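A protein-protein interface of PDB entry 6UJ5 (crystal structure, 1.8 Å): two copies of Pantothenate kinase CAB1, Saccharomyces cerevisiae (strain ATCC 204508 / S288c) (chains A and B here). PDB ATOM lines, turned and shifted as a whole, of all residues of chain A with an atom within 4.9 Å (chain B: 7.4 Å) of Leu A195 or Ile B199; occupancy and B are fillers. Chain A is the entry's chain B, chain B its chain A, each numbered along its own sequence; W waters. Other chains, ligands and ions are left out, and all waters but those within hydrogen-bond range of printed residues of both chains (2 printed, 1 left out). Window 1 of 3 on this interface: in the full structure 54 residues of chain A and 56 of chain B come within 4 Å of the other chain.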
ATOM      1  N   GLY A 190     -33.729  31.728 -19.187  1.00  0.00           N
ATOM      2  CA  GLY A 190     -32.536  31.070 -19.702  1.00  0.00           C
ATOM      3  C   GLY A 190     -32.424  29.621 -19.264  1.00  0.00           C
ATOM      4  O   GLY A 190     -31.939  28.769 -20.014  1.00  0.00           O
ATOM      5  N   THR A 191     -32.865  29.324 -18.039  1.00  0.00           N
ATOM      6  CA  THR A 191     -32.866  27.944 -17.554  1.00  0.00           C
ATOM      7  C   THR A 191     -33.881  27.096 -18.317  1.00  0.00           C
ATOM      8  O   THR A 191     -33.588  25.968 -18.737  1.00  0.00           O
ATOM      9  CB  THR A 191     -33.176  27.936 -16.053  1.00  0.00           C
ATOM     10  OG1 THR A 191     -32.352  28.913 -15.393  1.00  0.00           O
ATOM     11  CG2 THR A 191     -32.922  26.567 -15.457  1.00  0.00           C
ATOM     12  N   LEU A 192     -35.101  27.607 -18.459  1.00  0.00           N
ATOM     13  CA  LEU A 192     -36.124  26.879 -19.190  1.00  0.00           C
ATOM     14  C   LEU A 192     -35.697  26.653 -20.633  1.00  0.00           C
ATOM     15  O   LEU A 192     -35.798  25.535 -21.147  1.00  0.00           O
ATOM     16  CB  LEU A 192     -37.449  27.628 -19.129  1.00  0.00           C
ATOM     17  CG  LEU A 192     -38.602  26.992 -19.906  1.00  0.00           C
ATOM     18  CD1 LEU A 192     -39.039  25.661 -19.257  1.00  0.00           C
ATOM     19  CD2 LEU A 192     -39.763  27.950 -20.011  1.00  0.00           C
ATOM     20  N   TRP A 193     -35.203  27.706 -21.298  1.00  0.00           N
ATOM     21  CA  TRP A 193     -34.803  27.570 -22.700  1.00  0.00           C
ATOM     22  C   TRP A 193     -33.588  26.664 -22.838  1.00  0.00           C
ATOM     23  O   TRP A 193     -33.524  25.842 -23.761  1.00  0.00           O
ATOM     24  CB  TRP A 193     -34.504  28.946 -23.314  1.00  0.00           C
ATOM     25  CG  TRP A 193     -35.572  29.988 -23.076  1.00  0.00           C
ATOM     26  CD1 TRP A 193     -36.923  29.787 -23.042  1.00  0.00           C
ATOM     27  CD2 TRP A 193     -35.372  31.391 -22.816  1.00  0.00           C
ATOM     28  NE1 TRP A 193     -37.575  30.969 -22.785  1.00  0.00           N
ATOM     29  CE2 TRP A 193     -36.649  31.969 -22.638  1.00  0.00           C
ATOM     30  CE3 TRP A 193     -34.242  32.211 -22.711  1.00  0.00           C
ATOM     31  CZ2 TRP A 193     -36.827  33.330 -22.367  1.00  0.00           C
ATOM     32  CZ3 TRP A 193     -34.422  33.565 -22.437  1.00  0.00           C
ATOM     33  CH2 TRP A 193     -35.704  34.107 -22.272  1.00  0.00           C
ATOM     34  N   GLY A 194     -32.621  26.791 -21.925  1.00  0.00           N
ATOM     35  CA  GLY A 194     -31.425  25.970 -22.021  1.00  0.00           C
ATOM     36  C   GLY A 194     -31.723  24.491 -21.839  1.00  0.00           C
ATOM     37  O   GLY A 194     -31.238  23.650 -22.602  1.00  0.00           O
ATOM     38  N   LEU A 195     -32.537  24.158 -20.841  1.00  0.00           N
ATOM     39  CA  LEU A 195     -32.882  22.752 -20.599  1.00  0.00           C
ATOM     40  C   LEU A 195     -33.700  22.164 -21.747  1.00  0.00           C
ATOM     41  O   LEU A 195     -33.435  21.046 -22.199  1.00  0.00           O
ATOM     42  CB  LEU A 195     -33.654  22.639 -19.285  1.00  0.00           C
ATOM     43  CG  LEU A 195     -32.799  22.853 -18.040  1.00  0.00           C
ATOM     44  CD1 LEU A 195     -33.711  22.893 -16.833  1.00  0.00           C
ATOM     45  CD2 LEU A 195     -31.773  21.726 -17.910  1.00  0.00           C
ATOM     46  N   LEU A 196     -34.720  22.884 -22.217  1.00  0.00           N
ATOM     47  CA  LEU A 196     -35.588  22.299 -23.234  1.00  0.00           C
ATOM     48  C   LEU A 196     -34.922  22.261 -24.603  1.00  0.00           C
ATOM     49  O   LEU A 196     -35.165  21.341 -25.392  1.00  0.00           O
ATOM     50  CB  LEU A 196     -36.908  23.062 -23.308  1.00  0.00           C
ATOM     51  CG  LEU A 196     -37.790  22.923 -22.060  1.00  0.00           C
ATOM     52  CD1 LEU A 196     -39.058  23.740 -22.261  1.00  0.00           C
ATOM     53  CD2 LEU A 196     -38.119  21.447 -21.843  1.00  0.00           C
ATOM     54  N   SER A 197     -34.104  23.248 -24.933  1.00  0.00           N
ATOM     55  CA  SER A 197     -33.448  23.167 -26.231  1.00  0.00           C
ATOM     56  C   SER A 197     -32.477  21.992 -26.267  1.00  0.00           C
ATOM     57  O   SER A 197     -32.444  21.239 -27.246  1.00  0.00           O
ATOM     58  CB  SER A 197     -32.745  24.486 -26.557  1.00  0.00           C
ATOM     59  OG  SER A 197     -31.752  24.792 -25.609  1.00  0.00           O
ATOM     60  N   LEU A 198     -31.724  21.779 -25.187  1.00  0.00           N
ATOM     61  CA  LEU A 198     -30.820  20.633 -25.142  1.00  0.00           C
ATOM     62  C   LEU A 198     -31.593  19.316 -25.138  1.00  0.00           C
ATOM     63  O   LEU A 198     -31.285  18.401 -25.909  1.00  0.00           O
ATOM     64  CB  LEU A 198     -29.915  20.737 -23.911  1.00  0.00           C
ATOM     65  CG  LEU A 198     -28.887  19.621 -23.691  1.00  0.00           C
ATOM     66  CD1 LEU A 198     -27.975  19.462 -24.897  1.00  0.00           C
ATOM     67  CD2 LEU A 198     -28.064  19.913 -22.446  1.00  0.00           C
ATOM     68  N   ILE A 199     -32.599  19.194 -24.269  1.00  0.00           N
ATOM     69  CA  ILE A 199     -33.269  17.902 -24.112  1.00  0.00           C
ATOM     70  C   ILE A 199     -34.167  17.589 -25.308  1.00  0.00           C
ATOM     71  O   ILE A 199     -34.192  16.451 -25.795  1.00  0.00           O
ATOM     72  CB  ILE A 199     -34.063  17.878 -22.789  1.00  0.00           C
ATOM     73  CG1 ILE A 199     -33.110  17.857 -21.595  1.00  0.00           C
ATOM     74  CG2 ILE A 199     -34.988  16.651 -22.727  1.00  0.00           C
ATOM     75  CD1 ILE A 199     -33.809  18.219 -20.266  1.00  0.00           C
ATOM     76  N   THR A 200     -34.947  18.561 -25.781  1.00  0.00           N
ATOM     77  CA  THR A 200     -35.983  18.286 -26.778  1.00  0.00           C
ATOM     78  C   THR A 200     -35.609  18.745 -28.179  1.00  0.00           C
ATOM     79  O   THR A 200     -36.284  18.356 -29.148  1.00  0.00           O
ATOM     80  CB  THR A 200     -37.312  18.960 -26.394  1.00  0.00           C
ATOM     81  OG1 THR A 200     -37.217  20.371 -26.613  1.00  0.00           O
ATOM     82  CG2 THR A 200     -37.669  18.689 -24.928  1.00  0.00           C
ATOM     83  N   SER A 269     -22.143  15.626 -23.734  1.00  0.00           N
ATOM     84  CA  SER A 269     -23.489  15.266 -24.137  1.00  0.00           C
ATOM     85  C   SER A 269     -23.999  16.294 -25.138  1.00  0.00           C
ATOM     86  O   SER A 269     -23.537  17.437 -25.184  1.00  0.00           O
ATOM     87  CB  SER A 269     -24.444  15.177 -22.936  1.00  0.00           C
ATOM     88  OG  SER A 269     -24.261  13.958 -22.240  1.00  0.00           O
ATOM     89  N   ILE A 274     -28.725  12.617 -26.123  1.00  0.00           N
ATOM     90  CA  ILE A 274     -29.896  12.511 -25.260  1.00  0.00           C
ATOM     91  C   ILE A 274     -31.036  11.837 -26.006  1.00  0.00           C
ATOM     92  O   ILE A 274     -31.737  10.973 -25.465  1.00  0.00           O
ATOM     93  CB  ILE A 274     -30.310  13.903 -24.768  1.00  0.00           C
ATOM     94  CG1 ILE A 274     -29.195  14.502 -23.909  1.00  0.00           C
ATOM     95  CG2 ILE A 274     -31.633  13.808 -23.998  1.00  0.00           C
ATOM     96  CD1 ILE A 274     -29.406  15.970 -23.571  1.00  0.00           C
ATOM     97  N   LEU A 291     -41.371  21.186 -17.529  1.00  0.00           N
ATOM     98  CA  LEU A 291     -40.376  22.172 -17.120  1.00  0.00           C
ATOM     99  C   LEU A 291     -40.929  23.589 -17.174  1.00  0.00           C
ATOM    100  O   LEU A 291     -40.517  24.435 -16.371  1.00  0.00           O
ATOM    101  CB  LEU A 291     -39.104  22.053 -17.974  1.00  0.00           C
ATOM    102  CG  LEU A 291     -38.335  20.748 -17.725  1.00  0.00           C
ATOM    103  CD1 LEU A 291     -36.964  20.838 -18.371  1.00  0.00           C
ATOM    104  CD2 LEU A 291     -38.219  20.422 -16.220  1.00  0.00           C
ATOM    105  N   THR B 191     -36.139  15.944  -9.180  1.00  0.00           N
ATOM    106  CA  THR B 191     -35.891  16.821 -10.319  1.00  0.00           C
ATOM    107  C   THR B 191     -34.427  16.777 -10.727  1.00  0.00           C
ATOM    108  O   THR B 191     -34.096  16.667 -11.916  1.00  0.00           O
ATOM    109  CB  THR B 191     -36.293  18.253  -9.958  1.00  0.00           C
ATOM    110  OG1 THR B 191     -37.572  18.242  -9.305  1.00  0.00           O
ATOM    111  CG2 THR B 191     -36.377  19.107 -11.206  1.00  0.00           C
ATOM    112  N   TRP B 193     -32.055  14.431 -10.025  1.00  0.00           N
ATOM    113  CA  TRP B 193     -31.644  13.122 -10.539  1.00  0.00           C
ATOM    114  C   TRP B 193     -32.301  12.826 -11.885  1.00  0.00           C
ATOM    115  O   TRP B 193     -31.666  12.245 -12.775  1.00  0.00           O
ATOM    116  CB  TRP B 193     -31.972  12.016  -9.527  1.00  0.00           C
ATOM    117  CG  TRP B 193     -31.532  12.285  -8.094  1.00  0.00           C
ATOM    118  CD1 TRP B 193     -32.290  12.130  -6.967  1.00  0.00           C
ATOM    119  CD2 TRP B 193     -30.240  12.724  -7.642  1.00  0.00           C
ATOM    120  NE1 TRP B 193     -31.562  12.461  -5.853  1.00  0.00           N
ATOM    121  CE2 TRP B 193     -30.300  12.824  -6.238  1.00  0.00           C
ATOM    122  CE3 TRP B 193     -29.042  13.039  -8.284  1.00  0.00           C
ATOM    123  CZ2 TRP B 193     -29.207  13.233  -5.468  1.00  0.00           C
ATOM    124  CZ3 TRP B 193     -27.952  13.440  -7.514  1.00  0.00           C
ATOM    125  CH2 TRP B 193     -28.047  13.539  -6.125  1.00  0.00           C
ATOM    126  N   GLY B 194     -33.562  13.229 -12.057  1.00  0.00           N
ATOM    127  CA  GLY B 194     -34.228  13.035 -13.336  1.00  0.00           C
ATOM    128  C   GLY B 194     -33.587  13.826 -14.463  1.00  0.00           C
ATOM    129  O   GLY B 194     -33.319  13.289 -15.545  1.00  0.00           O
ATOM    130  N   LEU B 195     -33.325  15.115 -14.226  1.00  0.00           N
ATOM    131  CA  LEU B 195     -32.659  15.926 -15.248  1.00  0.00           C
ATOM    132  C   LEU B 195     -31.291  15.359 -15.593  1.00  0.00           C
ATOM    133  O   LEU B 195     -30.966  15.167 -16.769  1.00  0.00           O
ATOM    134  CB  LEU B 195     -32.521  17.370 -14.775  1.00  0.00           C
ATOM    135  CG  LEU B 195     -33.829  18.138 -14.770  1.00  0.00           C
ATOM    136  CD1 LEU B 195     -33.623  19.471 -14.076  1.00  0.00           C
ATOM    137  CD2 LEU B 195     -34.320  18.319 -16.207  1.00  0.00           C
ATOM    138  N   LEU B 196     -30.477  15.070 -14.577  1.00  0.00           N
ATOM    139  CA  LEU B 196     -29.110  14.636 -14.846  1.00  0.00           C
ATOM    140  C   LEU B 196     -29.082  13.262 -15.491  1.00  0.00           C
ATOM    141  O   LEU B 196     -28.247  13.005 -16.367  1.00  0.00           O
ATOM    142  CB  LEU B 196     -28.284  14.653 -13.562  1.00  0.00           C
ATOM    143  CG  LEU B 196     -28.005  16.075 -13.047  1.00  0.00           C
ATOM    144  CD1 LEU B 196     -27.066  16.023 -11.855  1.00  0.00           C
ATOM    145  CD2 LEU B 196     -27.417  16.970 -14.159  1.00  0.00           C
ATOM    146  N   SER B 197     -29.979  12.363 -15.074  1.00  0.00           N
ATOM    147  CA  SER B 197     -30.052  11.049 -15.711  1.00  0.00           C
ATOM    148  C   SER B 197     -30.356  11.174 -17.197  1.00  0.00           C
ATOM    149  O   SER B 197     -29.711  10.530 -18.039  1.00  0.00           O
ATOM    150  CB  SER B 197     -31.129  10.199 -15.026  1.00  0.00           C
ATOM    151  OG  SER B 197     -31.337   9.003 -15.751  1.00  0.00           O
ATOM    152  N   LEU B 198     -31.368  11.969 -17.537  1.00  0.00           N
ATOM    153  CA  LEU B 198     -31.758  12.104 -18.936  1.00  0.00           C
ATOM    154  C   LEU B 198     -30.679  12.805 -19.759  1.00  0.00           C
ATOM    155  O   LEU B 198     -30.383  12.394 -20.889  1.00  0.00           O
ATOM    156  CB  LEU B 198     -33.079  12.866 -19.022  1.00  0.00           C
ATOM    157  CG  LEU B 198     -33.710  12.997 -20.398  1.00  0.00           C
ATOM    158  CD1 LEU B 198     -33.942  11.631 -20.948  1.00  0.00           C
ATOM    159  CD2 LEU B 198     -35.020  13.742 -20.267  1.00  0.00           C
ATOM    160  N   ILE B 199     -30.083  13.865 -19.218  1.00  0.00           N
ATOM    161  CA  ILE B 199     -29.153  14.675 -20.004  1.00  0.00           C
ATOM    162  C   ILE B 199     -27.818  13.960 -20.183  1.00  0.00           C
ATOM    163  O   ILE B 199     -27.281  13.889 -21.298  1.00  0.00           O
ATOM    164  CB  ILE B 199     -28.959  16.049 -19.336  1.00  0.00           C
ATOM    165  CG1 ILE B 199     -30.228  16.883 -19.475  1.00  0.00           C
ATOM    166  CG2 ILE B 199     -27.803  16.786 -19.992  1.00  0.00           C
ATOM    167  CD1 ILE B 199     -30.197  18.155 -18.646  1.00  0.00           C
ATOM    168  N   THR B 200     -27.252  13.430 -19.094  1.00  0.00           N
ATOM    169  CA  THR B 200     -25.894  12.888 -19.118  1.00  0.00           C
ATOM    170  C   THR B 200     -25.836  11.376 -19.238  1.00  0.00           C
ATOM    171  O   THR B 200     -24.750  10.839 -19.481  1.00  0.00           O
ATOM    172  CB  THR B 200     -25.124  13.272 -17.850  1.00  0.00           C
ATOM    173  OG1 THR B 200     -25.606  12.492 -16.741  1.00  0.00           O
ATOM    174  CG2 THR B 200     -25.257  14.751 -17.559  1.00  0.00           C
ATOM    175  N   GLY B 201     -26.946  10.679 -19.046  1.00  0.00           N
ATOM    176  CA  GLY B 201     -26.938   9.234 -19.043  1.00  0.00           C
ATOM    177  C   GLY B 201     -26.425   8.602 -17.768  1.00  0.00           C
ATOM    178  O   GLY B 201     -26.347   7.371 -17.697  1.00  0.00           O
ATOM    179  N   ALA B 202     -26.075   9.399 -16.760  1.00  0.00           N
ATOM    180  CA  ALA B 202     -25.592   8.850 -15.502  1.00  0.00           C
ATOM    181  C   ALA B 202     -26.623   7.903 -14.905  1.00  0.00           C
ATOM    182  O   ALA B 202     -27.824   8.187 -14.897  1.00  0.00           O
ATOM    183  CB  ALA B 202     -25.286   9.972 -14.513  1.00  0.00           C
ATOM    184  N   TRP B 211     -19.238  13.629 -10.904  1.00  0.00           N
ATOM    185  CA  TRP B 211     -19.119  14.587 -12.004  1.00  0.00           C
ATOM    186  C   TRP B 211     -19.312  16.018 -11.509  1.00  0.00           C
ATOM    187  O   TRP B 211     -18.563  16.929 -11.882  1.00  0.00           O
ATOM    188  CB  TRP B 211     -20.155  14.262 -13.075  1.00  0.00           C
ATOM    189  CG  TRP B 211     -19.659  13.460 -14.224  1.00  0.00           C
ATOM    190  CD1 TRP B 211     -18.361  13.298 -14.629  1.00  0.00           C
ATOM    191  CD2 TRP B 211     -20.464  12.710 -15.139  1.00  0.00           C
ATOM    192  NE1 TRP B 211     -18.313  12.491 -15.749  1.00  0.00           N
ATOM    193  CE2 TRP B 211     -19.592  12.128 -16.085  1.00  0.00           C
ATOM    194  CE3 TRP B 211     -21.839  12.493 -15.263  1.00  0.00           C
ATOM    195  CZ2 TRP B 211     -20.053  11.324 -17.124  1.00  0.00           C
ATOM    196  CZ3 TRP B 211     -22.292  11.696 -16.299  1.00  0.00           C
ATOM    197  CH2 TRP B 211     -21.402  11.125 -17.217  1.00  0.00           C
ATOM    198  N   SER B 245     -28.913  29.938 -14.413  1.00  0.00           N
ATOM    199  CA  SER B 245     -28.451  28.556 -14.461  1.00  0.00           C
ATOM    200  C   SER B 245     -28.811  27.975 -15.814  1.00  0.00           C
ATOM    201  O   SER B 245     -29.952  28.113 -16.261  1.00  0.00           O
ATOM    202  CB  SER B 245     -29.107  27.731 -13.343  1.00  0.00           C
ATOM    203  OG  SER B 245     -28.678  28.149 -12.051  1.00  0.00           O
ATOM    204  N   PHE B 246     -27.842  27.343 -16.479  1.00  0.00           N
ATOM    205  CA  PHE B 246     -28.035  26.775 -17.811  1.00  0.00           C
ATOM    206  C   PHE B 246     -28.292  27.843 -18.867  1.00  0.00           C
ATOM    207  O   PHE B 246     -28.677  27.523 -19.993  1.00  0.00           O
ATOM    208  CB  PHE B 246     -29.170  25.736 -17.820  1.00  0.00           C
ATOM    209  CG  PHE B 246     -28.741  24.375 -18.290  1.00  0.00           C
ATOM    210  CD1 PHE B 246     -27.784  23.658 -17.601  1.00  0.00           C
ATOM    211  CD2 PHE B 246     -29.313  23.813 -19.422  1.00  0.00           C
ATOM    212  CE1 PHE B 246     -27.398  22.396 -18.045  1.00  0.00           C
ATOM    213  CE2 PHE B 246     -28.924  22.558 -19.870  1.00  0.00           C
ATOM    214  CZ  PHE B 246     -27.974  21.857 -19.185  1.00  0.00           C
ATOM    215  N   GLY B 247     -28.055  29.112 -18.542  1.00  0.00           N
ATOM    216  CA  GLY B 247     -28.409  30.193 -19.438  1.00  0.00           C
ATOM    217  C   GLY B 247     -27.547  30.294 -20.677  1.00  0.00           C
ATOM    218  O   GLY B 247     -27.936  30.979 -21.626  1.00  0.00           O
ATOM    219  N   VAL B 249     -26.741  27.653 -22.566  1.00  0.00           N
ATOM    220  CA  VAL B 249     -26.969  26.502 -23.433  1.00  0.00           C
ATOM    221  C   VAL B 249     -27.816  26.891 -24.639  1.00  0.00           C
ATOM    222  O   VAL B 249     -27.447  26.612 -25.785  1.00  0.00           O
ATOM    223  CB  VAL B 249     -27.591  25.362 -22.609  1.00  0.00           C
ATOM    224  CG1 VAL B 249     -27.950  24.173 -23.483  1.00  0.00           C
ATOM    225  CG2 VAL B 249     -26.620  24.951 -21.521  1.00  0.00           C
ATOM    226  N   PHE B 250     -28.938  27.579 -24.410  1.00  0.00           N
ATOM    227  CA  PHE B 250     -29.799  27.963 -25.533  1.00  0.00           C
ATOM    228  C   PHE B 250     -29.106  28.929 -26.495  1.00  0.00           C
ATOM    229  O   PHE B 250     -29.535  29.060 -27.644  1.00  0.00           O
ATOM    230  CB  PHE B 250     -31.111  28.565 -24.993  1.00  0.00           C
ATOM    231  CG  PHE B 250     -32.102  28.963 -26.052  1.00  0.00           C
ATOM    232  CD1 PHE B 250     -32.664  28.018 -26.887  1.00  0.00           C
ATOM    233  CD2 PHE B 250     -32.501  30.285 -26.180  1.00  0.00           C
ATOM    234  CE1 PHE B 250     -33.583  28.383 -27.856  1.00  0.00           C
ATOM    235  CE2 PHE B 250     -33.423  30.659 -27.143  1.00  0.00           C
ATOM    236  CZ  PHE B 250     -33.965  29.705 -27.981  1.00  0.00           C
ATOM    237  N   PHE B 282     -21.912  19.702 -24.742  1.00  0.00           N
ATOM    238  CA  PHE B 282     -21.722  20.275 -23.419  1.00  0.00           C
ATOM    239  C   PHE B 282     -21.140  19.222 -22.484  1.00  0.00           C
ATOM    240  O   PHE B 282     -21.485  18.038 -22.584  1.00  0.00           O
ATOM    241  CB  PHE B 282     -23.055  20.816 -22.874  1.00  0.00           C
ATOM    242  CG  PHE B 282     -23.713  21.819 -23.791  1.00  0.00           C
ATOM    243  CD1 PHE B 282     -23.361  23.152 -23.736  1.00  0.00           C
ATOM    244  CD2 PHE B 282     -24.633  21.406 -24.749  1.00  0.00           C
ATOM    245  CE1 PHE B 282     -23.931  24.074 -24.602  1.00  0.00           C
ATOM    246  CE2 PHE B 282     -25.215  22.322 -25.606  1.00  0.00           C
ATOM    247  CZ  PHE B 282     -24.863  23.662 -25.528  1.00  0.00           C
ATOM    248  N   LYS B 283     -20.258  19.652 -21.577  1.00  0.00           N
ATOM    249  CA  LYS B 283     -19.565  18.705 -20.705  1.00  0.00           C
ATOM    250  C   LYS B 283     -20.484  18.184 -19.606  1.00  0.00           C
ATOM    251  O   LYS B 283     -21.095  18.960 -18.869  1.00  0.00           O
ATOM    252  CB  LYS B 283     -18.340  19.342 -20.048  1.00  0.00           C
ATOM    253  CG  LYS B 283     -17.186  19.670 -20.955  1.00  0.00           C
ATOM    254  CD  LYS B 283     -15.962  19.962 -20.102  1.00  0.00           C
ATOM    255  CE  LYS B 283     -14.797  20.446 -20.932  1.00  0.00           C
ATOM    256  NZ  LYS B 283     -15.092  21.765 -21.556  1.00  0.00           N
ATOM    257  N   ASN B 284     -20.528  16.863 -19.461  1.00  0.00           N
ATOM    258  CA  ASN B 284     -21.295  16.245 -18.379  1.00  0.00           C
ATOM    259  C   ASN B 284     -20.895  16.728 -16.992  1.00  0.00           C
ATOM    260  O   ASN B 284     -21.794  17.026 -16.181  1.00  0.00           O
ATOM    261  CB  ASN B 284     -21.171  14.716 -18.490  1.00  0.00           C
ATOM    262  CG  ASN B 284     -21.942  14.159 -19.672  1.00  0.00           C
ATOM    263  OD1 ASN B 284     -22.980  14.696 -20.060  1.00  0.00           O
ATOM    264  ND2 ASN B 284     -21.434  13.094 -20.254  1.00  0.00           N
ATOM    265  N   ILE B 287     -22.436  20.208 -16.550  1.00  0.00           N
ATOM    266  CA  ILE B 287     -23.883  20.098 -16.432  1.00  0.00           C
ATOM    267  C   ILE B 287     -24.279  19.652 -15.032  1.00  0.00           C
ATOM    268  O   ILE B 287     -25.236  20.174 -14.448  1.00  0.00           O
ATOM    269  CB  ILE B 287     -24.413  19.114 -17.495  1.00  0.00           C
ATOM    270  CG1 ILE B 287     -24.199  19.678 -18.899  1.00  0.00           C
ATOM    271  CG2 ILE B 287     -25.872  18.799 -17.251  1.00  0.00           C
ATOM    272  CD1 ILE B 287     -24.502  18.651 -20.006  1.00  0.00           C
ATOM    273  N   CYS B 288     -23.587  18.642 -14.490  1.00  0.00           N
ATOM    274  CA  CYS B 288     -23.928  18.143 -13.160  1.00  0.00           C
ATOM    275  C   CYS B 288     -23.712  19.210 -12.092  1.00  0.00           C
ATOM    276  O   CYS B 288     -24.557  19.392 -11.205  1.00  0.00           O
ATOM    277  CB  CYS B 288     -23.103  16.901 -12.843  1.00  0.00           C
ATOM    278  SG  CYS B 288     -23.617  15.469 -13.838  1.00  0.00           S
ATOM    279  N   SER B 290     -23.674  22.505 -12.593  1.00  0.00           N
ATOM    280  CA  SER B 290     -24.691  23.538 -12.800  1.00  0.00           C
ATOM    281  C   SER B 290     -26.041  23.151 -12.183  1.00  0.00           C
ATOM    282  O   SER B 290     -26.652  23.942 -11.450  1.00  0.00           O
ATOM    283  CB  SER B 290     -24.838  23.835 -14.297  1.00  0.00           C
ATOM    284  OG  SER B 290     -26.031  24.572 -14.576  1.00  0.00           O
ATOM    285  N   LEU B 291     -26.542  21.940 -12.472  1.00  0.00           N
ATOM    286  CA  LEU B 291     -27.879  21.636 -11.976  1.00  0.00           C
ATOM    287  C   LEU B 291     -27.878  21.315 -10.487  1.00  0.00           C
ATOM    288  O   LEU B 291     -28.855  21.630  -9.800  1.00  0.00           O
ATOM    289  CB  LEU B 291     -28.511  20.490 -12.779  1.00  0.00           C
ATOM    290  CG  LEU B 291     -28.737  20.932 -14.233  1.00  0.00           C
ATOM    291  CD1 LEU B 291     -29.514  19.893 -15.050  1.00  0.00           C
ATOM    292  CD2 LEU B 291     -29.414  22.314 -14.307  1.00  0.00           C
HETATM  293  O   HOH W   1     -29.051  23.954 -26.848  1.00  0.00           O
HETATM  294  O   HOH W   2     -26.035  12.150 -23.168  1.00  0.00           O
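Leu A195 touches Ile B199, but with the chains exchanged Ile A199 does not touch Leu B195 (4.1 Å).
Leu A198 touches Ile B199, and with the chains exchanged Ile A199 touches Leu B198.
Ile B199 touches its own counterpart, Ile A199.
Positions printed for both chains: 191, 193, 194, 195, 196, 197, 198, 199, 200 and 291.
Of the 22 pairs that touch across the chains among the printed residues, 3 have their exchanged pair printed and touching as well.
The side-chain hydroxyl (OG1) of Thr B200 is in hydrogen-bond range of the backbone carbonyl oxygen (O) of Leu B196.
The side-chain hydroxyl of Thr B200 sits at hydrogen-bond distance from the backbone NH of Ala B202 (3.1 Å).
SG of Cys B288 lies within hydrogen-bond range of O of Asn B284.
The backbone carbonyl oxygen (O) of Trp A193 sits at hydrogen-bond distance from the side-chain hydroxyl (OG) of Ser A197.
O of Gly A194 sits at hydrogen-bond distance from OG of Ser A197.
Hydrophobic or aromatic side chains of chain B within 4 Å of the printed part of chain A: Leu B198, Ile B199, Phe B246, Val B249, Phe B250 and Phe B282.
Hydrophobic or aromatic side chains of chain A that line the printed part of chain B: Trp A193, Leu A195, Leu A198, Ile A199 and Ile A274.
Water W2 bridges the side-chain hydroxyl of Ser A269 (2.7 Å) and the backbone carbonyl oxygen of Ile B199 (2.8 Å).
Water W1 bridges OG of Ser A197 (3.1 Å) and O of Val B249 (3.3 Å).
Gly A190 touches Gly B247.
Phe B250 touches Trp A193.
Val B249 touches Gly A194.
Leu A195 touches Ile B199.
N of Leu A195 touches CD2 of Phe B246, 3.5 Å away.
Phe B250 touches Ser A197.
Leu A198 touches Val B249 (CB to CG1, 3.98 Å).
CD1 of Leu A198 touches CD2 of Phe B282, at 3.9 Å.
Ile A199 touches Ile B199.
Ile A274 touches Ile B199.
The side-chain hydroxyl (OG) of Ser A269 sits at hydrogen-bond distance from the backbone carbonyl oxygen (O) of Ile B199.
The backbone carbonyl oxygen (O) of Ser B245 sits at hydrogen-bond distance from the side-chain hydroxyl (OG1) of Thr A191 (2.7 Å).
The backbone NH of Ser A269 lies within hydrogen-bond range of the backbone carbonyl oxygen of Phe B282 (2.8 Å).
The side-chain hydroxyl (OG) of Ser A269 sits at hydrogen-bond distance from the side-chain amide oxygen (OD1) of Asn B284, at 2.6 Å.
O of Gly A190 sits close to O of Phe B246, at 3.5 Å.
Leu A195 touches two residues of chain B.
Of the printed residues of chain B, Leu A198 touches Ile B199, Phe B246, Val B249 and Phe B282.
Printed residues of chain A within 4 Å of Ile B199: Leu A195 (3.97 Å), Leu A198 (3.98 Å), Ile A199 (3.7 Å), Ser A269 (3.2 Å) and Ile A274 (3.3 Å).
Of the printed residues of chain A, Val B249 touches Gly A194 and Leu A198.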
